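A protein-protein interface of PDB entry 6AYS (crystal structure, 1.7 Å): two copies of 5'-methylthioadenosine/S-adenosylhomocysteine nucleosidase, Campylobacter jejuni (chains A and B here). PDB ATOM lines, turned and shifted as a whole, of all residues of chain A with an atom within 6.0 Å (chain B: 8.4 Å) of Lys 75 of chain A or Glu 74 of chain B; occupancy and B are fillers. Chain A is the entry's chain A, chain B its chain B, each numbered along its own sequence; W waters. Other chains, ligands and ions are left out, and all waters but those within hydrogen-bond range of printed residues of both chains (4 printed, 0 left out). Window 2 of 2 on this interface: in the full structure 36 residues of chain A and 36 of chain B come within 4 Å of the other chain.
The side-chain carboxylate of Glu 74 of chain A lies within hydrogen-bond range of a ring nitrogen (NE2) of His 38 of chain B (2.6 Å).
The side-chain amino group (NZ) of Lys 75 of chain A lies within hydrogen-bond range of the backbone carbonyl oxygen (O) of Glu 74 of chain B (3.2 Å).
The side-chain hydroxyl (OG) of Ser 70 of chain A sits at hydrogen-bond distance from the side-chain hydroxyl (OG) of Ser 70 of chain B (2.8 Å).
A ring nitrogen (NE2) of His 38 of chain A lies within hydrogen-bond range of the side-chain carboxylate (OE1) of Glu 74 of chain B (2.6 Å).
The side-chain amino group (NZ) of Lys 75 of chain B is in hydrogen-bond range of the backbone carbonyl oxygen (O) of Glu 74 of chain A, 3.3 Å away.
O of Val 71 of chain B lies within hydrogen-bond range of N of Phe 76 of chain B (3.1 Å).
N of Phe 76 of chain A sits at hydrogen-bond distance from O of Val 71 of chain A (3.1 Å).
His 38 of chain A touches Leu 194 of chain B.
Ala 39 of chain A touches Ala 193 of chain B (CA to O, 3.3 Å).
Leu 194 of chain B touches Ala 39 of chain A (CD2 to CB, 3.7 Å).
Leu 67 of chain A touches Thr 66 of chain B (N to CG2, 3.8 Å).
Leu 67 of chain A touches Ser 70 of chain B.
Leu 67 of chain A touches Ala 193 of chain B (CD2 to CB, 3.9 Å).
CD1 of Leu 67 of chain B touches OG of Ser 70 of chain A (3.8 Å).
CG2 of Val 71 of chain A touches OE1 of Glu 74 of chain B (3.6 Å).
Val 71 of chain B touches Glu 74 of chain A.
Glu 74 of chain A touches Glu 74 of chain B.
Of the printed residues of chain A, Glu 74 of chain B touches His 38 (2.6 Å), Val 71 (3.6 Å), Glu 74 (3.98 Å) and Lys 75 (3.2 Å).
Of the printed residues of chain A, Val 71 of chain B touches Glu 74 (3.5 Å).
Of the printed residues of chain A, Thr 66 of chain B touches Leu 67.
Of the printed residues of chain A, Leu 67 of chain B touches Ser 70 (3.8 Å).
Of the printed residues of chain A, His 38 of chain B touches Glu 74 (2.6 Å).
Ser 68 of chain B touches none of the printed residues of chain A.
The nearest residue of chain B that does not touch Lys 75 of chain A is Ile 73 of chain B (5.1 Å).
Of the 11 printed residues of chain A, 7 touch a printed residue of chain B.
Of the 20 printed residues of chain B, 9 touch a printed residue of chain A.
Printed residues of chain B that touch a printed residue of chain A: His 38, Thr 66, Leu 67, Ser 70, Val 71, Glu 74, Lys 75, Ala 193 and Leu 194.
Hydrophobic or aromatic side chains of chain B that line the printed part of chain A: His 38, Leu 67, Val 71, Ala 193 and Leu 194.
Among the printed residues, 15 pairs touch across the chains.
Among the printed residues, no Asp or Glu carboxylate lies within 4 Å of a Lys or Arg side-chain nitrogen of the other chain.
His 38 of chain A touches Glu 74 of chain B, and with the chains exchanged Glu 74 of chain A touches His 38 of chain B.
Leu 67 of chain A touches Ser 70 of chain B, and with the chains exchanged Ser 70 of chain A touches Leu 67 of chain B.
Glu 74 of chain A touches its own counterpart, Glu 74 of chain B.
Glu 74 of chain A touches Lys 75 of chain B, and with the chains exchanged Lys 75 of chain A touches Glu 74 of chain B.
Of the 15 pairs that touch across the chains among the printed residues, 10 have their exchanged pair printed and touching as well.
Water W4 lies within hydrogen-bond range of NZ of Lys 75 of chain A, O of Ile 73 of chain B and O of Glu 74 of chain B.
Water W1 lies within hydrogen-bond range of O of Ile 73 of chain A (2.9 Å), NZ of Lys 75 of chain B (3.0 Å) and O of Glu 74 of chain A (3.1 Å).
Water W2 lies within hydrogen-bond range of N of Ala 39 of chain A (2.9 Å), ND1 of His 38 of chain A (3.3 Å) and O of Ala 193 of chain B (3.4 Å).
Water W3 lies within hydrogen-bond range of O of Glu 74 of chain B (3.0 Å), NZ of Lys 75 of chain A (3.2 Å) and O of Glu 74 of chain A (3.3 Å).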
ATOM      1  N   HIS A  38     -25.072 -23.017   7.802  1.00  0.00           N
ATOM      2  CA  HIS A  38     -23.984 -22.290   7.170  1.00  0.00           C
ATOM      3  C   HIS A  38     -24.164 -22.345   5.663  1.00  0.00           C
ATOM      4  O   HIS A  38     -24.615 -23.357   5.140  1.00  0.00           O
ATOM      5  CB  HIS A  38     -22.629 -22.895   7.549  1.00  0.00           C
ATOM      6  CG  HIS A  38     -21.462 -22.067   7.119  1.00  0.00           C
ATOM      7  ND1 HIS A  38     -21.123 -20.898   7.752  1.00  0.00           N
ATOM      8  CD2 HIS A  38     -20.566 -22.223   6.116  1.00  0.00           C
ATOM      9  CE1 HIS A  38     -20.046 -20.383   7.186  1.00  0.00           C
ATOM     10  NE2 HIS A  38     -19.707 -21.152   6.169  1.00  0.00           N
ATOM     11  N   ALA A  39     -23.814 -21.256   4.977  1.00  0.00           N
ATOM     12  CA  ALA A  39     -23.896 -21.198   3.509  1.00  0.00           C
ATOM     13  C   ALA A  39     -25.292 -21.542   2.971  1.00  0.00           C
ATOM     14  O   ALA A  39     -25.425 -22.249   1.970  1.00  0.00           O
ATOM     15  CB  ALA A  39     -22.820 -22.097   2.902  1.00  0.00           C
ATOM     16  N   LEU A  67     -19.915 -24.914  -4.126  1.00  0.00           N
ATOM     17  CA  LEU A  67     -19.949 -24.182  -2.864  1.00  0.00           C
ATOM     18  C   LEU A  67     -19.820 -25.131  -1.678  1.00  0.00           C
ATOM     19  O   LEU A  67     -19.000 -24.885  -0.784  1.00  0.00           O
ATOM     20  CB  LEU A  67     -21.230 -23.346  -2.748  1.00  0.00           C
ATOM     21  CG  LEU A  67     -21.462 -22.605  -1.428  1.00  0.00           C
ATOM     22  CD1 LEU A  67     -20.308 -21.667  -1.093  1.00  0.00           C
ATOM     23  CD2 LEU A  67     -22.805 -21.901  -1.467  1.00  0.00           C
ATOM     24  N   SER A  70     -16.328 -26.621  -1.371  1.00  0.00           N
ATOM     25  CA  SER A  70     -15.430 -25.555  -0.927  1.00  0.00           C
ATOM     26  C   SER A  70     -15.591 -25.273   0.560  1.00  0.00           C
ATOM     27  O   SER A  70     -14.598 -25.112   1.269  1.00  0.00           O
ATOM     28  CB  SER A  70     -15.675 -24.264  -1.716  1.00  0.00           C
ATOM     29  OG  SER A  70     -14.640 -23.335  -1.458  1.00  0.00           O
ATOM     30  N   VAL A  71     -16.839 -25.214   1.022  1.00  0.00           N
ATOM     31  CA  VAL A  71     -17.145 -25.001   2.444  1.00  0.00           C
ATOM     32  C   VAL A  71     -16.607 -26.143   3.300  1.00  0.00           C
ATOM     33  O   VAL A  71     -15.964 -25.904   4.330  1.00  0.00           O
ATOM     34  CB  VAL A  71     -18.672 -24.817   2.665  1.00  0.00           C
ATOM     35  CG1 VAL A  71     -19.073 -24.977   4.119  1.00  0.00           C
ATOM     36  CG2 VAL A  71     -19.124 -23.461   2.150  1.00  0.00           C
ATOM     37  N   MET A  72     -16.861 -27.378   2.872  1.00  0.00           N
ATOM     38  CA  MET A  72     -16.431 -28.555   3.637  1.00  0.00           C
ATOM     39  C   MET A  72     -14.915 -28.604   3.835  1.00  0.00           C
ATOM     40  O   MET A  72     -14.446 -29.007   4.903  1.00  0.00           O
ATOM     41  CB  MET A  72     -16.939 -29.830   2.993  1.00  0.00           C
ATOM     42  CG  MET A  72     -18.428 -30.032   3.235  1.00  0.00           C
ATOM     43  SD  MET A  72     -19.189 -31.161   2.031  1.00  0.00           S
ATOM     44  CE  MET A  72     -20.024 -32.281   3.130  1.00  0.00           C
ATOM     45  N   ILE A  73     -14.168 -28.161   2.826  1.00  0.00           N
ATOM     46  CA  ILE A  73     -12.710 -28.139   2.878  1.00  0.00           C
ATOM     47  C   ILE A  73     -12.192 -26.860   3.539  1.00  0.00           C
ATOM     48  O   ILE A  73     -11.439 -26.930   4.521  1.00  0.00           O
ATOM     49  CB  ILE A  73     -12.101 -28.330   1.466  1.00  0.00           C
ATOM     50  CG1 ILE A  73     -12.489 -29.715   0.923  1.00  0.00           C
ATOM     51  CG2 ILE A  73     -10.577 -28.185   1.502  1.00  0.00           C
ATOM     52  CD1 ILE A  73     -12.266 -29.905  -0.561  1.00  0.00           C
ATOM     53  N   GLU A  74     -12.574 -25.698   3.012  1.00  0.00           N
ATOM     54  CA  GLU A  74     -11.996 -24.420   3.466  1.00  0.00           C
ATOM     55  C   GLU A  74     -12.452 -24.006   4.861  1.00  0.00           C
ATOM     56  O   GLU A  74     -11.644 -23.480   5.634  1.00  0.00           O
ATOM     57  CB  GLU A  74     -12.285 -23.286   2.471  1.00  0.00           C
ATOM     58  CG  GLU A  74     -11.753 -23.484   1.062  1.00  0.00           C
ATOM     59  CD  GLU A  74     -10.219 -23.437   1.000  1.00  0.00           C
ATOM     60  OE1 GLU A  74      -9.658 -22.456   0.463  1.00  0.00           O
ATOM     61  OE2 GLU A  74      -9.566 -24.391   1.483  1.00  0.00           O
ATOM     62  N   LYS A  75     -13.724 -24.227   5.185  1.00  0.00           N
ATOM     63  CA  LYS A  75     -14.254 -23.868   6.498  1.00  0.00           C
ATOM     64  C   LYS A  75     -14.152 -25.018   7.494  1.00  0.00           C
ATOM     65  O   LYS A  75     -13.699 -24.809   8.618  1.00  0.00           O
ATOM     66  CB  LYS A  75     -15.705 -23.382   6.405  1.00  0.00           C
ATOM     67  CG  LYS A  75     -16.267 -22.864   7.734  1.00  0.00           C
ATOM     68  CD  LYS A  75     -15.485 -21.696   8.350  1.00  0.00           C
ATOM     69  CE  LYS A  75     -15.212 -20.545   7.384  1.00  0.00           C
ATOM     70  NZ  LYS A  75     -14.351 -19.495   8.008  1.00  0.00           N
ATOM     71  N   PHE A  76     -14.581 -26.213   7.103  1.00  0.00           N
ATOM     72  CA  PHE A  76     -14.672 -27.341   8.048  1.00  0.00           C
ATOM     73  C   PHE A  76     -13.494 -28.323   8.004  1.00  0.00           C
ATOM     74  O   PHE A  76     -13.491 -29.314   8.724  1.00  0.00           O
ATOM     75  CB  PHE A  76     -16.021 -28.060   7.888  1.00  0.00           C
ATOM     76  CG  PHE A  76     -17.215 -27.172   8.145  1.00  0.00           C
ATOM     77  CD1 PHE A  76     -17.329 -26.468   9.318  1.00  0.00           C
ATOM     78  CD2 PHE A  76     -18.231 -27.053   7.195  1.00  0.00           C
ATOM     79  CE1 PHE A  76     -18.419 -25.632   9.564  1.00  0.00           C
ATOM     80  CE2 PHE A  76     -19.347 -26.252   7.422  1.00  0.00           C
ATOM     81  CZ  PHE A  76     -19.423 -25.515   8.604  1.00  0.00           C
ATOM     82  N   GLY A  77     -12.483 -28.026   7.197  1.00  0.00           N
ATOM     83  CA  GLY A  77     -11.207 -28.738   7.233  1.00  0.00           C
ATOM     84  C   GLY A  77     -11.203 -30.185   6.766  1.00  0.00           C
ATOM     85  O   GLY A  77     -10.336 -30.950   7.179  1.00  0.00           O
ATOM     86  N   HIS B  38      -2.901 -20.619  -3.977  1.00  0.00           N
ATOM     87  CA  HIS B  38      -3.948 -21.381  -3.309  1.00  0.00           C
ATOM     88  C   HIS B  38      -5.048 -21.711  -4.304  1.00  0.00           C
ATOM     89  O   HIS B  38      -5.329 -20.906  -5.185  1.00  0.00           O
ATOM     90  CB  HIS B  38      -4.539 -20.578  -2.141  1.00  0.00           C
ATOM     91  CG  HIS B  38      -5.446 -21.380  -1.267  1.00  0.00           C
ATOM     92  ND1 HIS B  38      -4.982 -22.345  -0.398  1.00  0.00           N
ATOM     93  CD2 HIS B  38      -6.795 -21.373  -1.138  1.00  0.00           C
ATOM     94  CE1 HIS B  38      -6.008 -22.900   0.223  1.00  0.00           C
ATOM     95  NE2 HIS B  38      -7.116 -22.309  -0.187  1.00  0.00           N
ATOM     96  N   THR B  66     -17.325 -19.631  -8.573  1.00  0.00           N
ATOM     97  CA  THR B  66     -17.883 -20.091  -7.291  1.00  0.00           C
ATOM     98  C   THR B  66     -16.760 -20.433  -6.315  1.00  0.00           C
ATOM     99  O   THR B  66     -16.788 -20.014  -5.158  1.00  0.00           O
ATOM    100  CB  THR B  66     -18.794 -21.315  -7.477  1.00  0.00           C
ATOM    101  OG1 THR B  66     -19.876 -20.968  -8.340  1.00  0.00           O
ATOM    102  CG2 THR B  66     -19.377 -21.790  -6.156  1.00  0.00           C
ATOM    103  N   LEU B  67     -15.780 -21.197  -6.792  1.00  0.00           N
ATOM    104  CA  LEU B  67     -14.653 -21.596  -5.957  1.00  0.00           C
ATOM    105  C   LEU B  67     -13.895 -20.374  -5.438  1.00  0.00           C
ATOM    106  O   LEU B  67     -13.613 -20.289  -4.241  1.00  0.00           O
ATOM    107  CB  LEU B  67     -13.712 -22.533  -6.723  1.00  0.00           C
ATOM    108  CG  LEU B  67     -12.398 -22.934  -6.041  1.00  0.00           C
ATOM    109  CD1 LEU B  67     -12.656 -23.609  -4.705  1.00  0.00           C
ATOM    110  CD2 LEU B  67     -11.590 -23.798  -6.997  1.00  0.00           C
ATOM    111  N   SER B  68     -13.574 -19.429  -6.328  1.00  0.00           N
ATOM    112  CA  SER B  68     -12.813 -18.239  -5.920  1.00  0.00           C
ATOM    113  C   SER B  68     -13.566 -17.369  -4.909  1.00  0.00           C
ATOM    114  O   SER B  68     -12.980 -16.932  -3.923  1.00  0.00           O
ATOM    115  CB  SER B  68     -12.391 -17.397  -7.107  1.00  0.00           C
ATOM    116  OG  SER B  68     -11.308 -18.012  -7.797  1.00  0.00           O
ATOM    117  N   ALA B  69     -14.856 -17.133  -5.141  1.00  0.00           N
ATOM    118  CA  ALA B  69     -15.674 -16.389  -4.167  1.00  0.00           C
ATOM    119  C   ALA B  69     -15.691 -17.100  -2.806  1.00  0.00           C
ATOM    120  O   ALA B  69     -15.541 -16.449  -1.765  1.00  0.00           O
ATOM    121  CB  ALA B  69     -17.094 -16.197  -4.681  1.00  0.00           C
ATOM    122  N   SER B  70     -15.857 -18.423  -2.828  1.00  0.00           N
ATOM    123  CA  SER B  70     -15.881 -19.226  -1.605  1.00  0.00           C
ATOM    124  C   SER B  70     -14.547 -19.149  -0.860  1.00  0.00           C
ATOM    125  O   SER B  70     -14.529 -19.006   0.360  1.00  0.00           O
ATOM    126  CB  SER B  70     -16.204 -20.689  -1.913  1.00  0.00           C
ATOM    127  OG  SER B  70     -16.471 -21.391  -0.716  1.00  0.00           O
ATOM    128  N   VAL B  71     -13.444 -19.250  -1.603  1.00  0.00           N
ATOM    129  CA  VAL B  71     -12.100 -19.145  -1.033  1.00  0.00           C
ATOM    130  C   VAL B  71     -11.868 -17.763  -0.416  1.00  0.00           C
ATOM    131  O   VAL B  71     -11.377 -17.653   0.716  1.00  0.00           O
ATOM    132  CB  VAL B  71     -11.010 -19.453  -2.095  1.00  0.00           C
ATOM    133  CG1 VAL B  71      -9.613 -18.993  -1.651  1.00  0.00           C
ATOM    134  CG2 VAL B  71     -10.973 -20.929  -2.436  1.00  0.00           C
ATOM    135  N   MET B  72     -12.229 -16.715  -1.146  1.00  0.00           N
ATOM    136  CA  MET B  72     -12.022 -15.346  -0.666  1.00  0.00           C
ATOM    137  C   MET B  72     -12.746 -15.055   0.644  1.00  0.00           C
ATOM    138  O   MET B  72     -12.213 -14.344   1.500  1.00  0.00           O
ATOM    139  CB  MET B  72     -12.416 -14.337  -1.740  1.00  0.00           C
ATOM    140  CG  MET B  72     -11.387 -14.268  -2.847  1.00  0.00           C
ATOM    141  SD  MET B  72     -12.027 -13.567  -4.357  1.00  0.00           S
ATOM    142  CE  MET B  72     -10.786 -12.312  -4.691  1.00  0.00           C
ATOM    143  N   ILE B  73     -13.931 -15.638   0.807  1.00  0.00           N
ATOM    144  CA  ILE B  73     -14.730 -15.466   2.020  1.00  0.00           C
ATOM    145  C   ILE B  73     -14.321 -16.468   3.106  1.00  0.00           C
ATOM    146  O   ILE B  73     -13.972 -16.062   4.225  1.00  0.00           O
ATOM    147  CB  ILE B  73     -16.242 -15.562   1.704  1.00  0.00           C
ATOM    148  CG1 ILE B  73     -16.641 -14.413   0.766  1.00  0.00           C
ATOM    149  CG2 ILE B  73     -17.078 -15.510   2.983  1.00  0.00           C
ATOM    150  CD1 ILE B  73     -17.987 -14.576   0.094  1.00  0.00           C
ATOM    151  N   GLU B  74     -14.364 -17.762   2.792  1.00  0.00           N
ATOM    152  CA  GLU B  74     -14.159 -18.808   3.811  1.00  0.00           C
ATOM    153  C   GLU B  74     -12.714 -18.910   4.296  1.00  0.00           C
ATOM    154  O   GLU B  74     -12.482 -19.127   5.484  1.00  0.00           O
ATOM    155  CB  GLU B  74     -14.633 -20.180   3.314  1.00  0.00           C
ATOM    156  CG  GLU B  74     -16.111 -20.272   2.932  1.00  0.00           C
ATOM    157  CD  GLU B  74     -17.049 -20.145   4.128  1.00  0.00           C
ATOM    158  OE1 GLU B  74     -17.677 -21.141   4.508  1.00  0.00           O
ATOM    159  OE2 GLU B  74     -17.164 -19.042   4.684  1.00  0.00           O
ATOM    160  N   LYS B  75     -11.749 -18.771   3.388  1.00  0.00           N
ATOM    161  CA  LYS B  75     -10.336 -18.859   3.749  1.00  0.00           C
ATOM    162  C   LYS B  75      -9.744 -17.498   4.090  1.00  0.00           C
ATOM    163  O   LYS B  75      -9.064 -17.370   5.105  1.00  0.00           O
ATOM    164  CB  LYS B  75      -9.513 -19.523   2.634  1.00  0.00           C
ATOM    165  CG  LYS B  75      -8.046 -19.759   2.988  1.00  0.00           C
ATOM    166  CD  LYS B  75      -7.840 -20.648   4.223  1.00  0.00           C
ATOM    167  CE  LYS B  75      -8.622 -21.965   4.187  1.00  0.00           C
ATOM    168  NZ  LYS B  75      -8.406 -22.786   5.408  1.00  0.00           N
ATOM    169  N   PHE B  76      -9.978 -16.494   3.246  1.00  0.00           N
ATOM    170  CA  PHE B  76      -9.320 -15.187   3.409  1.00  0.00           C
ATOM    171  C   PHE B  76     -10.168 -14.118   4.101  1.00  0.00           C
ATOM    172  O   PHE B  76      -9.720 -12.979   4.235  1.00  0.00           O
ATOM    173  CB  PHE B  76      -8.775 -14.702   2.056  1.00  0.00           C
ATOM    174  CG  PHE B  76      -7.757 -15.630   1.449  1.00  0.00           C
ATOM    175  CD1 PHE B  76      -6.635 -16.022   2.180  1.00  0.00           C
ATOM    176  CD2 PHE B  76      -7.903 -16.114   0.152  1.00  0.00           C
ATOM    177  CE1 PHE B  76      -5.691 -16.880   1.636  1.00  0.00           C
ATOM    178  CE2 PHE B  76      -6.953 -16.971  -0.396  1.00  0.00           C
ATOM    179  CZ  PHE B  76      -5.848 -17.347   0.342  1.00  0.00           C
ATOM    180  N   GLY B  77     -11.359 -14.479   4.556  1.00  0.00           N
ATOM    181  CA  GLY B  77     -12.157 -13.613   5.432  1.00  0.00           C
ATOM    182  C   GLY B  77     -12.734 -12.344   4.831  1.00  0.00           C
ATOM    183  O   GLY B  77     -12.994 -11.394   5.555  1.00  0.00           O
ATOM    184  N   ALA B  78     -12.951 -12.322   3.520  1.00  0.00           N
ATOM    185  CA  ALA B  78     -13.562 -11.156   2.870  1.00  0.00           C
ATOM    186  C   ALA B  78     -14.947 -10.874   3.462  1.00  0.00           C
ATOM    187  O   ALA B  78     -15.728 -11.794   3.688  1.00  0.00           O
ATOM    188  CB  ALA B  78     -13.668 -11.371   1.369  1.00  0.00           C
ATOM    189  N   GLN B  79     -15.215  -9.606   3.740  1.00  0.00           N
ATOM    190  CA  GLN B  79     -16.479  -9.155   4.344  1.00  0.00           C
ATOM    191  C   GLN B  79     -17.422  -8.484   3.349  1.00  0.00           C
ATOM    192  O   GLN B  79     -18.596  -8.325   3.633  1.00  0.00           O
ATOM    193  CB  GLN B  79     -16.184  -8.199   5.503  1.00  0.00           C
ATOM    194  CG  GLN B  79     -15.446  -8.858   6.653  1.00  0.00           C
ATOM    195  CD  GLN B  79     -14.862  -7.875   7.631  1.00  0.00           C
ATOM    196  OE1 GLN B  79     -14.095  -6.969   7.267  1.00  0.00           O
ATOM    197  NE2 GLN B  79     -15.215  -8.046   8.884  1.00  0.00           N
ATOM    198  N   VAL B 190     -22.950 -17.339  -3.959  1.00  0.00           N
ATOM    199  CA  VAL B 190     -21.987 -17.629  -2.896  1.00  0.00           C
ATOM    200  C   VAL B 190     -22.039 -16.547  -1.823  1.00  0.00           C
ATOM    201  O   VAL B 190     -22.145 -16.857  -0.630  1.00  0.00           O
ATOM    202  CB  VAL B 190     -20.538 -17.744  -3.426  1.00  0.00           C
ATOM    203  CG1 VAL B 190     -19.517 -17.809  -2.276  1.00  0.00           C
ATOM    204  CG2 VAL B 190     -20.373 -18.955  -4.321  1.00  0.00           C
ATOM    205  N   ALA B 193     -25.239 -16.670   0.217  1.00  0.00           N
ATOM    206  CA  ALA B 193     -25.206 -17.842   1.084  1.00  0.00           C
ATOM    207  C   ALA B 193     -24.329 -17.617   2.321  1.00  0.00           C
ATOM    208  O   ALA B 193     -24.691 -18.042   3.422  1.00  0.00           O
ATOM    209  CB  ALA B 193     -24.723 -19.063   0.309  1.00  0.00           C
ATOM    210  N   LEU B 194     -23.204 -16.928   2.132  1.00  0.00           N
ATOM    211  CA  LEU B 194     -22.251 -16.653   3.214  1.00  0.00           C
ATOM    212  C   LEU B 194     -22.450 -15.287   3.903  1.00  0.00           C
ATOM    213  O   LEU B 194     -21.603 -14.872   4.697  1.00  0.00           O
ATOM    214  CB  LEU B 194     -20.818 -16.799   2.686  1.00  0.00           C
ATOM    215  CG  LEU B 194     -20.478 -18.202   2.156  1.00  0.00           C
ATOM    216  CD1 LEU B 194     -19.121 -18.221   1.474  1.00  0.00           C
ATOM    217  CD2 LEU B 194     -20.528 -19.226   3.287  1.00  0.00           C
ATOM    218  N   LYS B 195     -23.568 -14.614   3.607  1.00  0.00           N
ATOM    219  CA  LYS B 195     -23.947 -13.334   4.227  1.00  0.00           C
ATOM    220  C   LYS B 195     -22.902 -12.227   4.024  1.00  0.00           C
ATOM    221  O   LYS B 195     -22.591 -11.462   4.944  1.00  0.00           O
ATOM    222  CB  LYS B 195     -24.279 -13.529   5.714  1.00  0.00           C
ATOM    223  CG  LYS B 195     -25.331 -14.608   5.948  1.00  0.00           C
ATOM    224  CD  LYS B 195     -25.841 -14.588   7.375  1.00  0.00           C
ATOM    225  CE  LYS B 195     -26.990 -15.569   7.559  1.00  0.00           C
ATOM    226  NZ  LYS B 195     -28.147 -15.249   6.676  1.00  0.00           N
ATOM    227  N   VAL B 196     -22.382 -12.156   2.804  1.00  0.00           N
ATOM    228  CA  VAL B 196     -21.408 -11.146   2.394  1.00  0.00           C
ATOM    229  C   VAL B 196     -22.087 -10.262   1.349  1.00  0.00           C
ATOM    230  O   VAL B 196     -22.606 -10.777   0.353  1.00  0.00           O
ATOM    231  CB  VAL B 196     -20.133 -11.820   1.826  1.00  0.00           C
ATOM    232  CG1 VAL B 196     -19.250 -10.828   1.098  1.00  0.00           C
ATOM    233  CG2 VAL B 196     -19.384 -12.536   2.947  1.00  0.00           C
HETATM  234  O   HOH W   1      -9.388 -25.566   5.969  1.00  0.00           O
HETATM  235  O   HOH W   2     -23.200 -18.784   6.336  1.00  0.00           O
HETATM  236  O   HOH W   3     -11.507 -20.873   7.728  1.00  0.00           O
HETATM  237  O   HOH W   4     -14.370 -16.956   6.969  1.00  0.00           O
